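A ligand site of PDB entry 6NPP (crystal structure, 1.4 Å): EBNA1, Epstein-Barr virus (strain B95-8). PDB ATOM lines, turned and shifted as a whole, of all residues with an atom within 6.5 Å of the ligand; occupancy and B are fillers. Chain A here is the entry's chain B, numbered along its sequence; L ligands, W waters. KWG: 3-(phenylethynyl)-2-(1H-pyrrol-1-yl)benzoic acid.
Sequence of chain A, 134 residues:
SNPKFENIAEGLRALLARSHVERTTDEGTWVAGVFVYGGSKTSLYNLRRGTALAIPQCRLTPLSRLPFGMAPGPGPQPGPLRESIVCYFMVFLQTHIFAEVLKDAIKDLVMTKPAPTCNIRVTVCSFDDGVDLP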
ATOM      1  N   LYS A   4      22.700  39.394  10.814  1.00  0.00           N
ATOM      2  CA  LYS A   4      22.833  37.941  10.825  1.00  0.00           C
ATOM      3  C   LYS A   4      21.771  37.290   9.961  1.00  0.00           C
ATOM      4  O   LYS A   4      22.078  36.461   9.092  1.00  0.00           O
ATOM      5  CB  LYS A   4      22.778  37.426  12.266  1.00  0.00           C
ATOM      6  CG  LYS A   4      22.782  35.896  12.422  1.00  0.00           C
ATOM      7  CD  LYS A   4      23.977  35.244  11.731  1.00  0.00           C
ATOM      8  CE  LYS A   4      25.286  35.616  12.376  1.00  0.00           C
ATOM      9  NZ  LYS A   4      25.341  35.343  13.858  1.00  0.00           N
ATOM     10  N   ASN A   7      22.362  38.113   6.341  1.00  0.00           N
ATOM     11  CA  ASN A   7      23.494  37.432   5.729  1.00  0.00           C
ATOM     12  C   ASN A   7      23.141  35.998   5.353  1.00  0.00           C
ATOM     13  O   ASN A   7      23.566  35.502   4.300  1.00  0.00           O
ATOM     14  CB  ASN A   7      24.687  37.469   6.698  1.00  0.00           C
ATOM     15  CG  ASN A   7      25.894  36.738   6.154  1.00  0.00           C
ATOM     16  OD1 ASN A   7      26.538  37.168   5.186  1.00  0.00           O
ATOM     17  ND2 ASN A   7      26.214  35.623   6.777  1.00  0.00           N
ATOM     18  N   ILE A   8      22.375  35.310   6.210  1.00  0.00           N
ATOM     19  CA  ILE A   8      21.903  33.969   5.895  1.00  0.00           C
ATOM     20  C   ILE A   8      21.000  34.021   4.671  1.00  0.00           C
ATOM     21  O   ILE A   8      21.151  33.242   3.717  1.00  0.00           O
ATOM     22  CB  ILE A   8      21.210  33.346   7.123  1.00  0.00           C
ATOM     23  CG1 ILE A   8      22.233  33.123   8.250  1.00  0.00           C
ATOM     24  CG2 ILE A   8      20.528  32.028   6.765  1.00  0.00           C
ATOM     25  CD1 ILE A   8      21.612  32.769   9.621  1.00  0.00           C
ATOM     26  N   ALA A   9      20.097  34.999   4.651  1.00  0.00           N
ATOM     27  CA  ALA A   9      19.239  35.170   3.484  1.00  0.00           C
ATOM     28  C   ALA A   9      20.056  35.389   2.219  1.00  0.00           C
ATOM     29  O   ALA A   9      19.774  34.791   1.174  1.00  0.00           O
ATOM     30  CB  ALA A   9      18.268  36.318   3.707  1.00  0.00           C
ATOM     31  N   GLU A  10      21.082  36.233   2.277  1.00  0.00           N
ATOM     32  CA  GLU A  10      21.890  36.457   1.079  1.00  0.00           C
ATOM     33  C   GLU A  10      22.592  35.176   0.629  1.00  0.00           C
ATOM     34  O   GLU A  10      22.688  34.904  -0.582  1.00  0.00           O
ATOM     35  CB  GLU A  10      22.909  37.572   1.308  1.00  0.00           C
ATOM     36  CG  GLU A  10      23.618  37.986  -0.001  1.00  0.00           C
ATOM     37  CD  GLU A  10      22.693  38.021  -1.237  1.00  0.00           C
ATOM     38  OE1 GLU A  10      21.685  38.784  -1.208  1.00  0.00           O
ATOM     39  OE2 GLU A  10      22.957  37.273  -2.216  1.00  0.00           O
ATOM     40  N   GLY A  11      23.126  34.404   1.572  1.00  0.00           N
ATOM     41  CA  GLY A  11      23.772  33.153   1.224  1.00  0.00           C
ATOM     42  C   GLY A  11      22.805  32.174   0.594  1.00  0.00           C
ATOM     43  O   GLY A  11      23.129  31.504  -0.399  1.00  0.00           O
ATOM     44  N   LEU A  12      21.592  32.085   1.138  1.00  0.00           N
ATOM     45  CA  LEU A  12      20.598  31.210   0.544  1.00  0.00           C
ATOM     46  C   LEU A  12      20.235  31.682  -0.853  1.00  0.00           C
ATOM     47  O   LEU A  12      20.162  30.880  -1.788  1.00  0.00           O
ATOM     48  CB  LEU A  12      19.347  31.197   1.416  1.00  0.00           C
ATOM     49  CG  LEU A  12      19.322  30.266   2.617  1.00  0.00           C
ATOM     50  CD1 LEU A  12      17.998  30.503   3.366  1.00  0.00           C
ATOM     51  CD2 LEU A  12      19.472  28.833   2.179  1.00  0.00           C
ATOM     52  N   LEU A  15      22.651  30.636  -3.564  1.00  0.00           N
ATOM     53  CA  LEU A  15      22.514  29.235  -3.941  1.00  0.00           C
ATOM     54  C   LEU A  15      21.231  29.010  -4.728  1.00  0.00           C
ATOM     55  O   LEU A  15      21.212  28.250  -5.702  1.00  0.00           O
ATOM     56  CB  LEU A  15      22.565  28.350  -2.702  1.00  0.00           C
ATOM     57  CG  LEU A  15      23.928  28.317  -2.007  1.00  0.00           C
ATOM     58  CD1 LEU A  15      23.829  27.941  -0.513  1.00  0.00           C
ATOM     59  CD2 LEU A  15      24.865  27.360  -2.736  1.00  0.00           C
ATOM     60  N   SER A  40      21.653  23.344  16.529  1.00  0.00           N
ATOM     61  CA  SER A  40      21.288  23.806  17.860  1.00  0.00           C
ATOM     62  C   SER A  40      20.023  24.626  17.715  1.00  0.00           C
ATOM     63  O   SER A  40      19.635  25.021  16.605  1.00  0.00           O
ATOM     64  CB  SER A  40      22.339  24.733  18.455  1.00  0.00           C
ATOM     65  OG  SER A  40      22.484  25.878  17.631  1.00  0.00           O
ATOM     66  N   THR A  42      19.529  27.737  18.537  1.00  0.00           N
ATOM     67  CA  THR A  42      19.810  29.067  18.024  1.00  0.00           C
ATOM     68  C   THR A  42      20.184  29.046  16.536  1.00  0.00           C
ATOM     69  O   THR A  42      19.764  29.917  15.771  1.00  0.00           O
ATOM     70  CB  THR A  42      20.901  29.710  18.879  1.00  0.00           C
ATOM     71  OG1 THR A  42      20.407  29.836  20.224  1.00  0.00           O
ATOM     72  CG2 THR A  42      21.234  31.059  18.350  1.00  0.00           C
ATOM     73  N   SER A  43      20.992  28.066  16.128  1.00  0.00           N
ATOM     74  CA  SER A  43      21.371  27.995  14.715  1.00  0.00           C
ATOM     75  C   SER A  43      20.152  27.722  13.835  1.00  0.00           C
ATOM     76  O   SER A  43      20.036  28.293  12.743  1.00  0.00           O
ATOM     77  CB  SER A  43      22.477  26.967  14.483  1.00  0.00           C
ATOM     78  OG  SER A  43      22.085  25.651  14.756  1.00  0.00           O
ATOM     79  N   LEU A  44      19.231  26.865  14.282  1.00  0.00           N
ATOM     80  CA  LEU A  44      17.998  26.636  13.538  1.00  0.00           C
ATOM     81  C   LEU A  44      17.148  27.900  13.481  1.00  0.00           C
ATOM     82  O   LEU A  44      16.537  28.193  12.456  1.00  0.00           O
ATOM     83  CB  LEU A  44      17.188  25.505  14.176  1.00  0.00           C
ATOM     84  CG  LEU A  44      17.602  24.073  13.913  1.00  0.00           C
ATOM     85  CD1 LEU A  44      16.698  23.145  14.766  1.00  0.00           C
ATOM     86  CD2 LEU A  44      17.490  23.763  12.430  1.00  0.00           C
ATOM     87  N   ASN A  46      18.155  30.996  13.554  1.00  0.00           N
ATOM     88  CA  ASN A  46      18.776  31.922  12.621  1.00  0.00           C
ATOM     89  C   ASN A  46      18.500  31.493  11.182  1.00  0.00           C
ATOM     90  O   ASN A  46      18.165  32.332  10.336  1.00  0.00           O
ATOM     91  CB  ASN A  46      20.276  31.978  12.889  1.00  0.00           C
ATOM     92  CG  ASN A  46      20.596  32.610  14.245  1.00  0.00           C
ATOM     93  OD1 ASN A  46      19.740  33.242  14.886  1.00  0.00           O
ATOM     94  ND2 ASN A  46      21.828  32.426  14.691  1.00  0.00           N
ATOM     95  N   LEU A  47      18.607  30.199  10.899  1.00  0.00           N
ATOM     96  CA  LEU A  47      18.295  29.720   9.548  1.00  0.00           C
ATOM     97  C   LEU A  47      16.833  29.994   9.196  1.00  0.00           C
ATOM     98  O   LEU A  47      16.514  30.379   8.063  1.00  0.00           O
ATOM     99  CB  LEU A  47      18.583  28.222   9.470  1.00  0.00           C
ATOM    100  CG  LEU A  47      18.314  27.597   8.094  1.00  0.00           C
ATOM    101  CD1 LEU A  47      19.130  28.221   6.993  1.00  0.00           C
ATOM    102  CD2 LEU A  47      18.581  26.086   8.151  1.00  0.00           C
ATOM    103  N   ASP A 108      23.956  22.837   1.165  1.00  0.00           N
ATOM    104  CA  ASP A 108      25.165  23.487   0.674  1.00  0.00           C
ATOM    105  C   ASP A 108      25.525  24.683   1.527  1.00  0.00           C
ATOM    106  O   ASP A 108      26.720  24.986   1.703  1.00  0.00           O
ATOM    107  CB  ASP A 108      24.968  23.914  -0.768  1.00  0.00           C
ATOM    108  CG  ASP A 108      25.022  22.745  -1.737  1.00  0.00           C
ATOM    109  OD1 ASP A 108      25.473  21.650  -1.319  1.00  0.00           O
ATOM    110  OD2 ASP A 108      24.609  22.936  -2.904  1.00  0.00           O
ATOM    111  N   LEU A 109      24.545  25.376   2.087  1.00  0.00           N
ATOM    112  CA  LEU A 109      24.831  26.551   2.888  1.00  0.00           C
ATOM    113  C   LEU A 109      25.466  26.171   4.213  1.00  0.00           C
ATOM    114  O   LEU A 109      26.475  26.760   4.633  1.00  0.00           O
ATOM    115  CB  LEU A 109      23.547  27.344   3.139  1.00  0.00           C
ATOM    116  CG  LEU A 109      23.784  28.712   3.803  1.00  0.00           C
ATOM    117  CD1 LEU A 109      24.398  29.662   2.787  1.00  0.00           C
ATOM    118  CD2 LEU A 109      22.500  29.300   4.363  1.00  0.00           C
ATOM    119  N   VAL A 110      24.849  25.224   4.928  1.00  0.00           N
ATOM    120  CA  VAL A 110      25.278  24.974   6.299  1.00  0.00           C
ATOM    121  C   VAL A 110      26.615  24.262   6.344  1.00  0.00           C
ATOM    122  O   VAL A 110      27.323  24.367   7.357  1.00  0.00           O
ATOM    123  CB  VAL A 110      24.214  24.234   7.128  1.00  0.00           C
ATOM    124  CG1 VAL A 110      22.936  25.015   7.155  1.00  0.00           C
ATOM    125  CG2 VAL A 110      23.993  22.822   6.615  1.00  0.00           C
ATOM    126  N   THR A 112      29.238  25.041   4.973  1.00  0.00           N
ATOM    127  CA  THR A 112      30.327  26.007   4.912  1.00  0.00           C
ATOM    128  C   THR A 112      30.661  26.588   6.284  1.00  0.00           C
ATOM    129  O   THR A 112      31.610  27.372   6.404  1.00  0.00           O
ATOM    130  CB  THR A 112      30.027  27.151   3.938  1.00  0.00           C
ATOM    131  OG1 THR A 112      28.969  27.955   4.475  1.00  0.00           O
ATOM    132  CG2 THR A 112      29.658  26.614   2.555  1.00  0.00           C
ATOM    133  N   LYS A 113      29.942  26.193   7.318  1.00  0.00           N
ATOM    134  CA  LYS A 113      30.077  26.799   8.634  1.00  0.00           C
ATOM    135  C   LYS A 113      30.529  25.747   9.637  1.00  0.00           C
ATOM    136  O   LYS A 113      30.356  24.544   9.416  1.00  0.00           O
ATOM    137  CB  LYS A 113      28.718  27.363   9.076  1.00  0.00           C
ATOM    138  CG  LYS A 113      28.308  28.583   8.298  1.00  0.00           C
ATOM    139  CD  LYS A 113      29.138  29.789   8.731  1.00  0.00           C
ATOM    140  CE  LYS A 113      28.662  31.042   7.996  1.00  0.00           C
ATOM    141  NZ  LYS A 113      29.481  32.241   8.354  1.00  0.00           N
ATOM    142  N   PRO A 114      31.143  26.161  10.748  1.00  0.00           N
ATOM    143  CA  PRO A 114      31.524  25.191  11.779  1.00  0.00           C
ATOM    144  C   PRO A 114      30.322  24.742  12.605  1.00  0.00           C
ATOM    145  O   PRO A 114      29.219  25.303  12.524  1.00  0.00           O
ATOM    146  CB  PRO A 114      32.538  25.952  12.643  1.00  0.00           C
ATOM    147  CG  PRO A 114      32.199  27.374  12.458  1.00  0.00           C
ATOM    148  CD  PRO A 114      31.578  27.534  11.072  1.00  0.00           C
ATOM    149  N   PRO A 116      27.831  24.424  15.626  1.00  0.00           N
ATOM    150  CA  PRO A 116      26.812  23.404  15.321  1.00  0.00           C
ATOM    151  C   PRO A 116      26.054  23.583  14.004  1.00  0.00           C
ATOM    152  O   PRO A 116      25.282  22.702  13.625  1.00  0.00           O
ATOM    153  CB  PRO A 116      25.843  23.536  16.482  1.00  0.00           C
ATOM    154  CG  PRO A 116      25.898  25.011  16.811  1.00  0.00           C
ATOM    155  CD  PRO A 116      27.358  25.370  16.648  1.00  0.00           C
ATOM    156  N   THR A 117      26.289  24.710  13.309  1.00  0.00           N
ATOM    157  CA  THR A 117      25.527  25.021  12.101  1.00  0.00           C
ATOM    158  C   THR A 117      25.594  23.880  11.104  1.00  0.00           C
ATOM    159  O   THR A 117      24.590  23.527  10.470  1.00  0.00           O
ATOM    160  CB  THR A 117      26.102  26.293  11.483  1.00  0.00           C
ATOM    161  OG1 THR A 117      26.064  27.352  12.443  1.00  0.00           O
ATOM    162  CG2 THR A 117      25.341  26.705  10.230  1.00  0.00           C
ATOM    163  N   ILE A 120      23.049  20.878  11.141  1.00  0.00           N
ATOM    164  CA  ILE A 120      21.671  21.012  10.723  1.00  0.00           C
ATOM    165  C   ILE A 120      21.420  20.000   9.586  1.00  0.00           C
ATOM    166  O   ILE A 120      22.257  19.836   8.707  1.00  0.00           O
ATOM    167  CB  ILE A 120      21.389  22.437  10.268  1.00  0.00           C
ATOM    168  CG1 ILE A 120      21.452  23.376  11.483  1.00  0.00           C
ATOM    169  CG2 ILE A 120      20.042  22.518   9.578  1.00  0.00           C
ATOM    170  CD1 ILE A 120      21.328  24.853  11.090  1.00  0.00           C
HETATM  171  C22 KWG L   1      25.821  32.858   4.967  1.00  0.00           C
HETATM  172  C20 KWG L   1      27.263  32.613   3.088  1.00  0.00           C
HETATM  173  C11 KWG L   1      26.445  30.828  11.030  1.00  0.00           C
HETATM  174  C12 KWG L   1      27.297  31.905  11.200  1.00  0.00           C
HETATM  175  C13 KWG L   1      26.749  32.969  10.485  1.00  0.00           C
HETATM  176  C17 KWG L   1      26.117  31.561   5.303  1.00  0.00           C
HETATM  177  C02 KWG L   1      23.904  30.069  12.372  1.00  0.00           C
HETATM  178  C04 KWG L   1      23.663  29.775  10.913  1.00  0.00           C
HETATM  179  C05 KWG L   1      22.641  28.904  10.605  1.00  0.00           C
HETATM  180  C06 KWG L   1      22.368  28.576   9.305  1.00  0.00           C
HETATM  181  C07 KWG L   1      23.118  29.149   8.284  1.00  0.00           C
HETATM  182  C08 KWG L   1      24.130  30.022   8.614  1.00  0.00           C
HETATM  183  C09 KWG L   1      24.444  30.354   9.909  1.00  0.00           C
HETATM  184  C14 KWG L   1      25.598  32.477   9.884  1.00  0.00           C
HETATM  185  C15 KWG L   1      24.938  30.583   7.480  1.00  0.00           C
HETATM  186  C16 KWG L   1      25.469  30.991   6.533  1.00  0.00           C
HETATM  187  C18 KWG L   1      26.983  30.769   4.567  1.00  0.00           C
HETATM  188  C19 KWG L   1      27.559  31.325   3.442  1.00  0.00           C
HETATM  189  C21 KWG L   1      26.405  33.391   3.843  1.00  0.00           C
HETATM  190  N10 KWG L   1      25.453  31.200  10.231  1.00  0.00           N
HETATM  191  O01 KWG L   1      23.723  31.239  12.788  1.00  0.00           O
HETATM  192  O03 KWG L   1      24.275  29.122  13.116  1.00  0.00           O
HETATM  193  O   HOH W   1      25.488  32.663  14.498  1.00  0.00           O
HETATM  194  O   HOH W   2      25.022  29.414  15.767  1.00  0.00           O
HETATM  195  O   HOH W   3      30.330  30.211   5.417  1.00  0.00           O
HETATM  196  O   HOH W   4      29.809  30.496  12.890  1.00  0.00           O
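OG1 of Thr 117 sits at hydrogen-bond distance from O03 of the ligand, at 2.6 Å.
ND2 of Asn 46 lies within hydrogen-bond range of O01 of the ligand (2.9 Å).
The backbone carbonyl oxygen (O) of Leu 109 is in hydrogen-bond range of the side-chain hydroxyl (OG1) of Thr 112 (2.8 Å).
OG of Ser 43 is in hydrogen-bond range of OG of Ser 40.
O of Thr 42 sits close to ND2 of Asn 46.
Lys 4 touches the ligand.
Asn 7 touches the ligand (ND2 to C22, 3.3 Å).
Ile 8 touches the ligand.
Gly 11 touches the ligand.
Ser 43 touches the ligand (CB to O03, 3.1 Å).
Leu 47 touches the ligand.
CD1 of Leu 109 touches C18 of the ligand, 3.3 Å away.
Thr 112 touches the ligand (OG1 to C18, 3.4 Å).
Lys 113 touches the ligand (CE to C16, 3.5 Å).
Hydrophobic or aromatic side chains that line the ligand: Ile 8, Leu 47 and Leu 109.
Water W1 bridges NZ of Lys 4 (2.8 Å) and O01 of the ligand (2.8 Å).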
